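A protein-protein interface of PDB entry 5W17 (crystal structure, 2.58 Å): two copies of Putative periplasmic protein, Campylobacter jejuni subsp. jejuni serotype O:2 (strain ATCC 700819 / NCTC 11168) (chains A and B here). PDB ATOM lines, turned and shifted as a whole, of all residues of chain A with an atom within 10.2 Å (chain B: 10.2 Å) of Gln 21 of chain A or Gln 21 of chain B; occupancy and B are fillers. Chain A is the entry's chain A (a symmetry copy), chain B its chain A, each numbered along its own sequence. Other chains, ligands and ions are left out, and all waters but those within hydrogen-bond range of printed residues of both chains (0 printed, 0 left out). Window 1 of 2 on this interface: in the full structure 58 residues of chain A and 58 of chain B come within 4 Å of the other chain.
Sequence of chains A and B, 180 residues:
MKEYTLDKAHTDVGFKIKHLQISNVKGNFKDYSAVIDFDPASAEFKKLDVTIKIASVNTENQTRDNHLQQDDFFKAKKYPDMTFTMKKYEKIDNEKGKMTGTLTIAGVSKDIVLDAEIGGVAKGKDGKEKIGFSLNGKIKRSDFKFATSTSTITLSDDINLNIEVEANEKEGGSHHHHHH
O of Ile 17 of chain B lies within hydrogen-bond range of N of Val 25 of chain A, at 2.7 Å.
The backbone carbonyl oxygen of Lys 18 of chain B is in hydrogen-bond range of the backbone NH of Ser 156 of chain A.
N of His 19 of chain B is in hydrogen-bond range of O of Ser 23 of chain A (2.8 Å).
The backbone NH of Leu 20 of chain B is in hydrogen-bond range of the backbone carbonyl oxygen of Thr 154 of chain A, at 2.8 Å.
O of Gln 21 of chain B lies within hydrogen-bond range of N of Gln 21 of chain A (2.9 Å).
The backbone carbonyl oxygen (O) of Ser 23 of chain B sits at hydrogen-bond distance from the backbone NH (N) of His 19 of chain A.
The backbone NH (N) of Val 25 of chain B is in hydrogen-bond range of the backbone carbonyl oxygen (O) of Ile 17 of chain A, 2.7 Å away.
The backbone carbonyl oxygen (O) of Thr 154 of chain B lies within hydrogen-bond range of the backbone NH (N) of Leu 20 of chain A (2.8 Å).
The backbone carbonyl oxygen (O) of Lys 18 of chain A is in hydrogen-bond range of the backbone NH (N) of Ser 156 of chain B (2.8 Å).
NE2 of His 19 of chain B lies within hydrogen-bond range of NE2 of Gln 21 of chain B (3.4 Å).
NE2 of His 19 of chain A is in hydrogen-bond range of NE2 of Gln 21 of chain A (3.4 Å).
Ser 23 of chain B touches Ile 17 of chain A.
Ile 17 of chain A touches Ser 156 of chain B (CD1 to O, 3.3 Å).
Lys 18 of chain A touches Leu 155 of chain B.
O of His 19 of chain A touches O of Gln 21 of chain B (3.7 Å).
His 19 of chain B touches Ile 22 of chain A.
Ser 23 of chain A touches Ile 17 of chain B.
O of Ser 23 of chain A touches CA of Lys 18 of chain B (3.4 Å).
Val 25 of chain A touches His 19 of chain B.
His 19 of chain B touches Leu 155 of chain A (CB to CD1, 3.8 Å).
Ser 156 of chain A touches Ile 17 of chain B (O to CD1, 3.3 Å).
Of chain B, only His 19, Leu 20 and Gln 21 come within 4 Å of Gln 21 of chain A.
Of chain A, only His 19, Leu 20 and Gln 21 come within 4 Å of Gln 21 of chain B.
Of chain B, only Gln 21 (3.4 Å), Ile 22 (3.8 Å), Ile 153 (3.6 Å) and Thr 154 (2.8 Å) come within 4 Å of Leu 20 of chain A.
Printed residues of chain B within 4 Å of Ile 22 of chain A: His 19 and Leu 20.
Of chain A, only Gln 21, Ile 22, Ile 153 and Thr 154 come within 4 Å of Leu 20 of chain B.
Of chain A, only His 19 (3.5 Å) and Leu 20 (3.8 Å) come within 4 Å of Ile 22 of chain B.
Ser 23 of chain B touches just these residues of chain A: Ile 17, Lys 18 and His 19.
Of the printed residues of chain B, His 19 of chain A touches Gln 21, Ile 22, Ser 23, Val 25, Thr 154 and Leu 155.
Of the printed residues of chain B, Ile 153 of chain A touches Leu 20 (3.6 Å).
Of the printed residues of chain A, Thr 154 of chain B touches His 19 (2.9 Å) and Leu 20 (2.8 Å).
Of the printed residues of chain A, Ile 153 of chain B touches Leu 20 (3.6 Å).
The nearest residue of chain A that does not touch Gln 21 of chain B is Ser 23 of chain A (4.6 Å).
Of the 16 printed residues of chain A, 13 touch a printed residue of chain B.
Printed residues of chain A that touch a printed residue of chain B: Ile 17, Lys 18, His 19, Leu 20, Gln 21, Ile 22, Ser 23, Asn 24, Val 25, Ile 153, Thr 154, Leu 155 and Ser 156.
Among the printed residues, 39 pairs touch across the chains.
Among the printed residues, no Asp or Glu carboxylate lies within 4 Å of a Lys or Arg side-chain nitrogen of the other chain.
Ile 17 of chain A touches Ser 23 of chain B, and with the chains exchanged Ser 23 of chain A touches Ile 17 of chain B.
Lys 18 of chain A touches Asn 24 of chain B, and with the chains exchanged Asn 24 of chain A touches Lys 18 of chain B.
Lys 18 of chain A touches Leu 155 of chain B, and with the chains exchanged Leu 155 of chain A touches Lys 18 of chain B.
Leu 20 of chain A touches Gln 21 of chain B, and with the chains exchanged Gln 21 of chain A touches Leu 20 of chain B.
Positions printed for both chains: 17, 18, 19, 20, 21, 22, 23, 24, 25, 61, 63, 64, 153, 154, 155 and 156.
Of the 39 pairs that touch across the chains among the printed residues, 39 have their exchanged pair printed and touching as well.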
ATOM      1  N   ILE A  17     -18.069  23.538  19.867  1.00  0.00           N
ATOM      2  CA  ILE A  17     -16.627  23.248  19.957  1.00  0.00           C
ATOM      3  C   ILE A  17     -16.280  21.985  19.148  1.00  0.00           C
ATOM      4  O   ILE A  17     -17.023  20.979  19.183  1.00  0.00           O
ATOM      5  CB  ILE A  17     -16.104  23.216  21.420  1.00  0.00           C
ATOM      6  CG1 ILE A  17     -14.618  22.912  21.433  1.00  0.00           C
ATOM      7  CG2 ILE A  17     -16.892  22.247  22.307  1.00  0.00           C
ATOM      8  CD1 ILE A  17     -13.949  23.260  22.723  1.00  0.00           C
ATOM      9  N   LYS A  18     -15.184  22.056  18.393  1.00  0.00           N
ATOM     10  CA  LYS A  18     -14.784  20.928  17.560  1.00  0.00           C
ATOM     11  C   LYS A  18     -13.996  19.913  18.397  1.00  0.00           C
ATOM     12  O   LYS A  18     -13.073  20.293  19.156  1.00  0.00           O
ATOM     13  CB  LYS A  18     -13.948  21.409  16.366  1.00  0.00           C
ATOM     14  CG  LYS A  18     -14.725  21.975  15.178  1.00  0.00           C
ATOM     15  CD  LYS A  18     -13.752  22.787  14.326  1.00  0.00           C
ATOM     16  CE  LYS A  18     -14.228  23.008  12.892  1.00  0.00           C
ATOM     17  NZ  LYS A  18     -15.184  24.151  12.779  1.00  0.00           N
ATOM     18  N   HIS A  19     -14.379  18.636  18.286  1.00  0.00           N
ATOM     19  CA  HIS A  19     -13.518  17.542  18.742  1.00  0.00           C
ATOM     20  C   HIS A  19     -13.372  16.348  17.795  1.00  0.00           C
ATOM     21  O   HIS A  19     -14.244  16.079  16.958  1.00  0.00           O
ATOM     22  CB  HIS A  19     -13.859  17.087  20.168  1.00  0.00           C
ATOM     23  CG  HIS A  19     -15.008  16.127  20.276  1.00  0.00           C
ATOM     24  ND1 HIS A  19     -16.128  16.193  19.469  1.00  0.00           N
ATOM     25  CD2 HIS A  19     -15.232  15.114  21.156  1.00  0.00           C
ATOM     26  CE1 HIS A  19     -16.979  15.243  19.820  1.00  0.00           C
ATOM     27  NE2 HIS A  19     -16.460  14.577  20.845  1.00  0.00           N
ATOM     28  N   LEU A  20     -12.245  15.653  17.969  1.00  0.00           N
ATOM     29  CA  LEU A  20     -11.942  14.396  17.317  1.00  0.00           C
ATOM     30  C   LEU A  20     -12.461  13.190  18.077  1.00  0.00           C
ATOM     31  O   LEU A  20     -12.487  13.178  19.311  1.00  0.00           O
ATOM     32  CB  LEU A  20     -10.443  14.273  17.176  1.00  0.00           C
ATOM     33  CG  LEU A  20      -9.820  15.352  16.300  1.00  0.00           C
ATOM     34  CD1 LEU A  20      -8.320  15.134  16.241  1.00  0.00           C
ATOM     35  CD2 LEU A  20     -10.424  15.342  14.906  1.00  0.00           C
ATOM     36  N   GLN A  21     -12.885  12.183  17.312  1.00  0.00           N
ATOM     37  CA  GLN A  21     -13.277  10.870  17.821  1.00  0.00           C
ATOM     38  C   GLN A  21     -12.662   9.762  16.965  1.00  0.00           C
ATOM     39  O   GLN A  21     -12.814   9.735  15.733  1.00  0.00           O
ATOM     40  CB  GLN A  21     -14.786  10.729  17.848  1.00  0.00           C
ATOM     41  CG  GLN A  21     -15.475  11.807  18.658  1.00  0.00           C
ATOM     42  CD  GLN A  21     -16.795  11.347  19.255  1.00  0.00           C
ATOM     43  OE1 GLN A  21     -17.774  11.133  18.529  1.00  0.00           O
ATOM     44  NE2 GLN A  21     -16.837  11.206  20.597  1.00  0.00           N
ATOM     45  N   ILE A  22     -11.942   8.870  17.642  1.00  0.00           N
ATOM     46  CA  ILE A  22     -11.374   7.655  17.061  1.00  0.00           C
ATOM     47  C   ILE A  22     -12.461   6.584  17.032  1.00  0.00           C
ATOM     48  O   ILE A  22     -13.258   6.490  17.958  1.00  0.00           O
ATOM     49  CB  ILE A  22     -10.137   7.199  17.873  1.00  0.00           C
ATOM     50  CG1 ILE A  22      -9.273   6.194  17.079  1.00  0.00           C
ATOM     51  CG2 ILE A  22     -10.540   6.714  19.271  1.00  0.00           C
ATOM     52  CD1 ILE A  22      -7.771   6.291  17.337  1.00  0.00           C
ATOM     53  N   SER A  23     -12.528   5.834  15.935  1.00  0.00           N
ATOM     54  CA  SER A  23     -13.440   4.688  15.787  1.00  0.00           C
ATOM     55  C   SER A  23     -12.839   3.699  14.787  1.00  0.00           C
ATOM     56  O   SER A  23     -12.002   4.065  13.945  1.00  0.00           O
ATOM     57  CB  SER A  23     -14.859   5.122  15.366  1.00  0.00           C
ATOM     58  OG  SER A  23     -14.895   5.608  14.032  1.00  0.00           O
ATOM     59  N   ASN A  24     -13.248   2.442  14.911  1.00  0.00           N
ATOM     60  CA  ASN A  24     -12.860   1.395  13.968  1.00  0.00           C
ATOM     61  C   ASN A  24     -13.833   1.357  12.795  1.00  0.00           C
ATOM     62  O   ASN A  24     -15.039   1.305  13.017  1.00  0.00           O
ATOM     63  CB  ASN A  24     -12.871   0.029  14.673  1.00  0.00           C
ATOM     64  CG  ASN A  24     -11.519  -0.355  15.242  1.00  0.00           C
ATOM     65  OD1 ASN A  24     -11.334  -0.383  16.456  1.00  0.00           O
ATOM     66  ND2 ASN A  24     -10.565  -0.665  14.364  1.00  0.00           N
ATOM     67  N   VAL A  25     -13.331   1.394  11.558  1.00  0.00           N
ATOM     68  CA  VAL A  25     -14.126   0.859  10.436  1.00  0.00           C
ATOM     69  C   VAL A  25     -13.932  -0.664  10.412  1.00  0.00           C
ATOM     70  O   VAL A  25     -12.788  -1.143  10.330  1.00  0.00           O
ATOM     71  CB  VAL A  25     -13.734   1.421   9.059  1.00  0.00           C
ATOM     72  CG1 VAL A  25     -14.830   1.093   8.049  1.00  0.00           C
ATOM     73  CG2 VAL A  25     -13.496   2.915   9.133  1.00  0.00           C
ATOM     74  N   ASN A  61     -22.064   0.687   4.905  1.00  0.00           N
ATOM     75  CA  ASN A  61     -22.252   2.086   4.554  1.00  0.00           C
ATOM     76  C   ASN A  61     -21.995   2.146   3.062  1.00  0.00           C
ATOM     77  O   ASN A  61     -20.876   1.856   2.621  1.00  0.00           O
ATOM     78  CB  ASN A  61     -21.252   2.953   5.352  1.00  0.00           C
ATOM     79  CG  ASN A  61     -20.917   4.278   4.666  1.00  0.00           C
ATOM     80  OD1 ASN A  61     -20.866   4.381   3.437  1.00  0.00           O
ATOM     81  ND2 ASN A  61     -20.652   5.298   5.470  1.00  0.00           N
ATOM     82  N   THR A  63     -22.031   4.825   0.716  1.00  0.00           N
ATOM     83  CA  THR A  63     -21.198   5.906   0.177  1.00  0.00           C
ATOM     84  C   THR A  63     -19.679   5.666   0.369  1.00  0.00           C
ATOM     85  O   THR A  63     -18.891   6.034  -0.512  1.00  0.00           O
ATOM     86  CB  THR A  63     -21.663   7.323   0.637  1.00  0.00           C
ATOM     87  OG1 THR A  63     -21.983   7.311   2.037  1.00  0.00           O
ATOM     88  CG2 THR A  63     -22.908   7.791  -0.154  1.00  0.00           C
ATOM     89  N   ARG A  64     -19.288   5.022   1.480  1.00  0.00           N
ATOM     90  CA  ARG A  64     -17.866   4.707   1.763  1.00  0.00           C
ATOM     91  C   ARG A  64     -17.401   3.545   0.898  1.00  0.00           C
ATOM     92  O   ARG A  64     -16.325   3.586   0.299  1.00  0.00           O
ATOM     93  CB  ARG A  64     -17.626   4.375   3.244  1.00  0.00           C
ATOM     94  CG  ARG A  64     -16.187   4.543   3.723  1.00  0.00           C
ATOM     95  CD  ARG A  64     -15.905   3.558   4.843  1.00  0.00           C
ATOM     96  NE  ARG A  64     -16.386   4.013   6.157  1.00  0.00           N
ATOM     97  CZ  ARG A  64     -17.358   3.436   6.885  1.00  0.00           C
ATOM     98  NH1 ARG A  64     -18.012   2.368   6.457  1.00  0.00           N
ATOM     99  NH2 ARG A  64     -17.701   3.949   8.059  1.00  0.00           N
ATOM    100  N   ILE A 153      -2.490   9.895   9.997  1.00  0.00           N
ATOM    101  CA  ILE A 153      -3.248  10.488  11.092  1.00  0.00           C
ATOM    102  C   ILE A 153      -4.725  10.174  10.995  1.00  0.00           C
ATOM    103  O   ILE A 153      -5.260   9.514  11.880  1.00  0.00           O
ATOM    104  CB  ILE A 153      -3.082  12.003  11.157  1.00  0.00           C
ATOM    105  CG1 ILE A 153      -1.603  12.381  11.312  1.00  0.00           C
ATOM    106  CG2 ILE A 153      -3.882  12.550  12.324  1.00  0.00           C
ATOM    107  CD1 ILE A 153      -1.271  13.811  10.904  1.00  0.00           C
ATOM    108  N   THR A 154      -5.373  10.651   9.937  1.00  0.00           N
ATOM    109  CA  THR A 154      -6.812  10.440   9.682  1.00  0.00           C
ATOM    110  C   THR A 154      -7.235   8.956   9.725  1.00  0.00           C
ATOM    111  O   THR A 154      -8.261   8.605  10.319  1.00  0.00           O
ATOM    112  CB  THR A 154      -7.185  11.004   8.280  1.00  0.00           C
ATOM    113  OG1 THR A 154      -6.568  12.286   8.113  1.00  0.00           O
ATOM    114  CG2 THR A 154      -8.749  11.044   8.010  1.00  0.00           C
ATOM    115  N   LEU A 155      -6.455   8.115   9.034  1.00  0.00           N
ATOM    116  CA  LEU A 155      -6.723   6.687   8.846  1.00  0.00           C
ATOM    117  C   LEU A 155      -5.441   6.014   9.214  1.00  0.00           C
ATOM    118  O   LEU A 155      -4.371   6.436   8.758  1.00  0.00           O
ATOM    119  CB  LEU A 155      -7.026   6.393   7.404  1.00  0.00           C
ATOM    120  CG  LEU A 155      -7.408   4.977   7.036  1.00  0.00           C
ATOM    121  CD1 LEU A 155      -8.838   4.696   7.442  1.00  0.00           C
ATOM    122  CD2 LEU A 155      -7.266   4.801   5.531  1.00  0.00           C
ATOM    123  N   SER A 156      -5.550   4.990  10.056  1.00  0.00           N
ATOM    124  CA  SER A 156      -4.393   4.355  10.664  1.00  0.00           C
ATOM    125  C   SER A 156      -3.521   3.664   9.595  1.00  0.00           C
ATOM    126  O   SER A 156      -4.050   3.109   8.608  1.00  0.00           O
ATOM    127  CB  SER A 156      -4.901   3.330  11.675  1.00  0.00           C
ATOM    128  OG  SER A 156      -3.851   2.513  12.134  1.00  0.00           O
ATOM    129  N   ILE B  17     -10.027  -1.119  10.653  1.00  0.00           N
ATOM    130  CA  ILE B  17      -9.029  -0.038  10.577  1.00  0.00           C
ATOM    131  C   ILE B  17      -9.497   1.186  11.385  1.00  0.00           C
ATOM    132  O   ILE B  17     -10.688   1.565  11.339  1.00  0.00           O
ATOM    133  CB  ILE B  17      -8.609   0.299   9.119  1.00  0.00           C
ATOM    134  CG1 ILE B  17      -7.583   1.417   9.120  1.00  0.00           C
ATOM    135  CG2 ILE B  17      -9.806   0.626   8.220  1.00  0.00           C
ATOM    136  CD1 ILE B  17      -6.825   1.532   7.838  1.00  0.00           C
ATOM    137  N   LYS B  18      -8.575   1.768  12.151  1.00  0.00           N
ATOM    138  CA  LYS B  18      -8.921   2.914  12.985  1.00  0.00           C
ATOM    139  C   LYS B  18      -8.870   4.201  12.152  1.00  0.00           C
ATOM    140  O   LYS B  18      -7.891   4.437  11.404  1.00  0.00           O
ATOM    141  CB  LYS B  18      -7.974   3.011  14.189  1.00  0.00           C
ATOM    142  CG  LYS B  18      -8.284   2.093  15.370  1.00  0.00           C
ATOM    143  CD  LYS B  18      -7.029   2.002  16.236  1.00  0.00           C
ATOM    144  CE  LYS B  18      -7.299   1.539  17.665  1.00  0.00           C
ATOM    145  NZ  LYS B  18      -7.404   0.053  17.772  1.00  0.00           N
ATOM    146  N   HIS B  19      -9.929   5.011  12.255  1.00  0.00           N
ATOM    147  CA  HIS B  19      -9.869   6.403  11.804  1.00  0.00           C
ATOM    148  C   HIS B  19     -10.461   7.453  12.749  1.00  0.00           C
ATOM    149  O   HIS B  19     -11.334   7.156  13.576  1.00  0.00           O
ATOM    150  CB  HIS B  19     -10.398   6.577  10.373  1.00  0.00           C
ATOM    151  CG  HIS B  19     -11.890   6.681  10.250  1.00  0.00           C
ATOM    152  ND1 HIS B  19     -12.767   5.967  11.046  1.00  0.00           N
ATOM    153  CD2 HIS B  19     -12.656   7.373   9.364  1.00  0.00           C
ATOM    154  CE1 HIS B  19     -14.009   6.240  10.683  1.00  0.00           C
ATOM    155  NE2 HIS B  19     -13.969   7.086   9.662  1.00  0.00           N
ATOM    156  N   LEU B  20      -9.954   8.677  12.584  1.00  0.00           N
ATOM    157  CA  LEU B  20     -10.452   9.871  13.236  1.00  0.00           C
ATOM    158  C   LEU B  20     -11.573  10.546  12.466  1.00  0.00           C
ATOM    159  O   LEU B  20     -11.587  10.544  11.232  1.00  0.00           O
ATOM    160  CB  LEU B  20      -9.312  10.849  13.391  1.00  0.00           C
ATOM    161  CG  LEU B  20      -8.184  10.338  14.277  1.00  0.00           C
ATOM    162  CD1 LEU B  20      -7.097  11.393  14.351  1.00  0.00           C
ATOM    163  CD2 LEU B  20      -8.693   9.987  15.665  1.00  0.00           C
ATOM    164  N   GLN B  21     -12.514  11.110  13.223  1.00  0.00           N
ATOM    165  CA  GLN B  21     -13.596  11.945  12.705  1.00  0.00           C
ATOM    166  C   GLN B  21     -13.757  13.201  13.564  1.00  0.00           C
ATOM    167  O   GLN B  21     -13.908  13.129  14.794  1.00  0.00           O
ATOM    168  CB  GLN B  21     -14.901  11.175  12.662  1.00  0.00           C
ATOM    169  CG  GLN B  21     -14.819   9.901  11.849  1.00  0.00           C
ATOM    170  CD  GLN B  21     -16.151   9.501  11.237  1.00  0.00           C
ATOM    171  OE1 GLN B  21     -17.077   9.098  11.952  1.00  0.00           O
ATOM    172  NE2 GLN B  21     -16.254   9.595   9.894  1.00  0.00           N
ATOM    173  N   ILE B  22     -13.690  14.348  12.891  1.00  0.00           N
ATOM    174  CA  ILE B  22     -13.948  15.662  13.474  1.00  0.00           C
ATOM    175  C   ILE B  22     -15.457  15.893  13.489  1.00  0.00           C
ATOM    176  O   ILE B  22     -16.148  15.505  12.554  1.00  0.00           O
ATOM    177  CB  ILE B  22     -13.205  16.761  12.674  1.00  0.00           C
ATOM    178  CG1 ILE B  22     -13.104  18.079  13.473  1.00  0.00           C
ATOM    179  CG2 ILE B  22     -13.801  16.921  11.270  1.00  0.00           C
ATOM    180  CD1 ILE B  22     -11.827  18.881  13.231  1.00  0.00           C
ATOM    181  N   SER B  23     -15.963  16.457  14.582  1.00  0.00           N
ATOM    182  CA  SER B  23     -17.375  16.850  14.717  1.00  0.00           C
ATOM    183  C   SER B  23     -17.478  18.000  15.720  1.00  0.00           C
ATOM    184  O   SER B  23     -16.594  18.192  16.571  1.00  0.00           O
ATOM    185  CB  SER B  23     -18.274  15.665  15.125  1.00  0.00           C
ATOM    186  OG  SER B  23     -18.032  15.245  16.460  1.00  0.00           O
ATOM    187  N   ASN B  24     -18.546  18.779  15.587  1.00  0.00           N
ATOM    188  CA  ASN B  24     -18.855  19.852  16.531  1.00  0.00           C
ATOM    189  C   ASN B  24     -19.677  19.308  17.694  1.00  0.00           C
ATOM    190  O   ASN B  24     -20.682  18.644  17.459  1.00  0.00           O
ATOM    191  CB  ASN B  24     -19.658  20.954  15.822  1.00  0.00           C
ATOM    192  CG  ASN B  24     -18.781  22.060  15.265  1.00  0.00           C
ATOM    193  OD1 ASN B  24     -18.636  22.195  14.052  1.00  0.00           O
ATOM    194  ND2 ASN B  24     -18.200  22.867  16.152  1.00  0.00           N
ATOM    195  N   VAL B  25     -19.262  19.568  18.936  1.00  0.00           N
ATOM    196  CA  VAL B  25     -20.231  19.531  20.047  1.00  0.00           C
ATOM    197  C   VAL B  25     -20.968  20.879  20.068  1.00  0.00           C
ATOM    198  O   VAL B  25     -20.322  21.938  20.161  1.00  0.00           O
ATOM    199  CB  VAL B  25     -19.599  19.303  21.430  1.00  0.00           C
ATOM    200  CG1 VAL B  25     -20.689  18.921  22.428  1.00  0.00           C
ATOM    201  CG2 VAL B  25     -18.529  18.231  21.365  1.00  0.00           C
ATOM    202  N   ASN B  61     -26.819  14.997  25.496  1.00  0.00           N
ATOM    203  CA  ASN B  61     -26.153  13.753  25.849  1.00  0.00           C
ATOM    204  C   ASN B  61     -25.926  13.850  27.345  1.00  0.00           C
ATOM    205  O   ASN B  61     -25.194  14.739  27.796  1.00  0.00           O
ATOM    206  CB  ASN B  61     -24.827  13.639  25.065  1.00  0.00           C
ATOM    207  CG  ASN B  61     -23.786  12.761  25.759  1.00  0.00           C
ATOM    208  OD1 ASN B  61     -23.697  12.703  26.989  1.00  0.00           O
ATOM    209  ND2 ASN B  61     -22.965  12.093  24.961  1.00  0.00           N
ATOM    210  N   THR B  63     -24.408  11.651  29.699  1.00  0.00           N
ATOM    211  CA  THR B  63     -23.105  11.262  30.250  1.00  0.00           C
ATOM    212  C   THR B  63     -22.014  12.347  30.073  1.00  0.00           C
ATOM    213  O   THR B  63     -21.169  12.509  30.963  1.00  0.00           O
ATOM    214  CB  THR B  63     -22.646   9.843  29.790  1.00  0.00           C
ATOM    215  OG1 THR B  63     -22.899   9.669  28.387  1.00  0.00           O
ATOM    216  CG2 THR B  63     -23.388   8.731  30.569  1.00  0.00           C
ATOM    217  N   ARG B  64     -22.063  13.103  28.964  1.00  0.00           N
ATOM    218  CA  ARG B  64     -21.093  14.192  28.694  1.00  0.00           C
ATOM    219  C   ARG B  64     -21.408  15.404  29.560  1.00  0.00           C
ATOM    220  O   ARG B  64     -20.518  15.999  30.171  1.00  0.00           O
ATOM    221  CB  ARG B  64     -21.078  14.607  27.215  1.00  0.00           C
ATOM    222  CG  ARG B  64     -19.810  15.317  26.752  1.00  0.00           C
ATOM    223  CD  ARG B  64     -20.147  16.283  25.631  1.00  0.00           C
ATOM    224  NE  ARG B  64     -20.256  15.637  24.313  1.00  0.00           N
ATOM    225  CZ  ARG B  64     -21.374  15.537  23.574  1.00  0.00           C
ATOM    226  NH1 ARG B  64     -22.534  16.017  23.991  1.00  0.00           N
ATOM    227  NH2 ARG B  64     -21.339  14.925  22.398  1.00  0.00           N
ATOM    228  N   ILE B 153      -5.512  19.035  20.637  1.00  0.00           N
ATOM    229  CA  ILE B 153      -5.766  18.113  19.536  1.00  0.00           C
ATOM    230  C   ILE B 153      -7.148  17.502  19.617  1.00  0.00           C
ATOM    231  O   ILE B 153      -7.959  17.726  18.724  1.00  0.00           O
ATOM    232  CB  ILE B 153      -4.744  16.984  19.479  1.00  0.00           C
ATOM    233  CG1 ILE B 153      -3.323  17.545  19.340  1.00  0.00           C
ATOM    234  CG2 ILE B 153      -5.059  16.076  18.305  1.00  0.00           C
ATOM    235  CD1 ILE B 153      -2.219  16.581  19.756  1.00  0.00           C
ATOM    236  N   THR B 154      -7.404  16.731  20.670  1.00  0.00           N
ATOM    237  CA  THR B 154      -8.697  16.058  20.910  1.00  0.00           C
ATOM    238  C   THR B 154      -9.909  17.012  20.857  1.00  0.00           C
ATOM    239  O   THR B 154     -10.939  16.696  20.252  1.00  0.00           O
ATOM    240  CB  THR B 154      -8.682  15.378  22.309  1.00  0.00           C
ATOM    241  OG1 THR B 154      -7.433  14.700  22.487  1.00  0.00           O
ATOM    242  CG2 THR B 154      -9.928  14.427  22.563  1.00  0.00           C
ATOM    243  N   LEU B 155      -9.777  18.149  21.553  1.00  0.00           N
ATOM    244  CA  LEU B 155     -10.835  19.147  21.734  1.00  0.00           C
ATOM    245  C   LEU B 155     -10.187  20.446  21.377  1.00  0.00           C
ATOM    246  O   LEU B 155      -9.076  20.729  21.846  1.00  0.00           O
ATOM    247  CB  LEU B 155     -11.266  19.203  23.172  1.00  0.00           C
ATOM    248  CG  LEU B 155     -12.410  20.124  23.531  1.00  0.00           C
ATOM    249  CD1 LEU B 155     -13.728  19.515  23.110  1.00  0.00           C
ATOM    250  CD2 LEU B 155     -12.414  20.345  25.037  1.00  0.00           C
ATOM    251  N   SER B 156     -10.867  21.214  20.530  1.00  0.00           N
ATOM    252  CA  SER B 156     -10.295  22.409  19.933  1.00  0.00           C
ATOM    253  C   SER B 156     -10.006  23.476  21.008  1.00  0.00           C
ATOM    254  O   SER B 156     -10.770  23.612  21.987  1.00  0.00           O
ATOM    255  CB  SER B 156     -11.299  22.944  18.913  1.00  0.00           C
ATOM    256  OG  SER B 156     -10.922  24.223  18.462  1.00  0.00           O
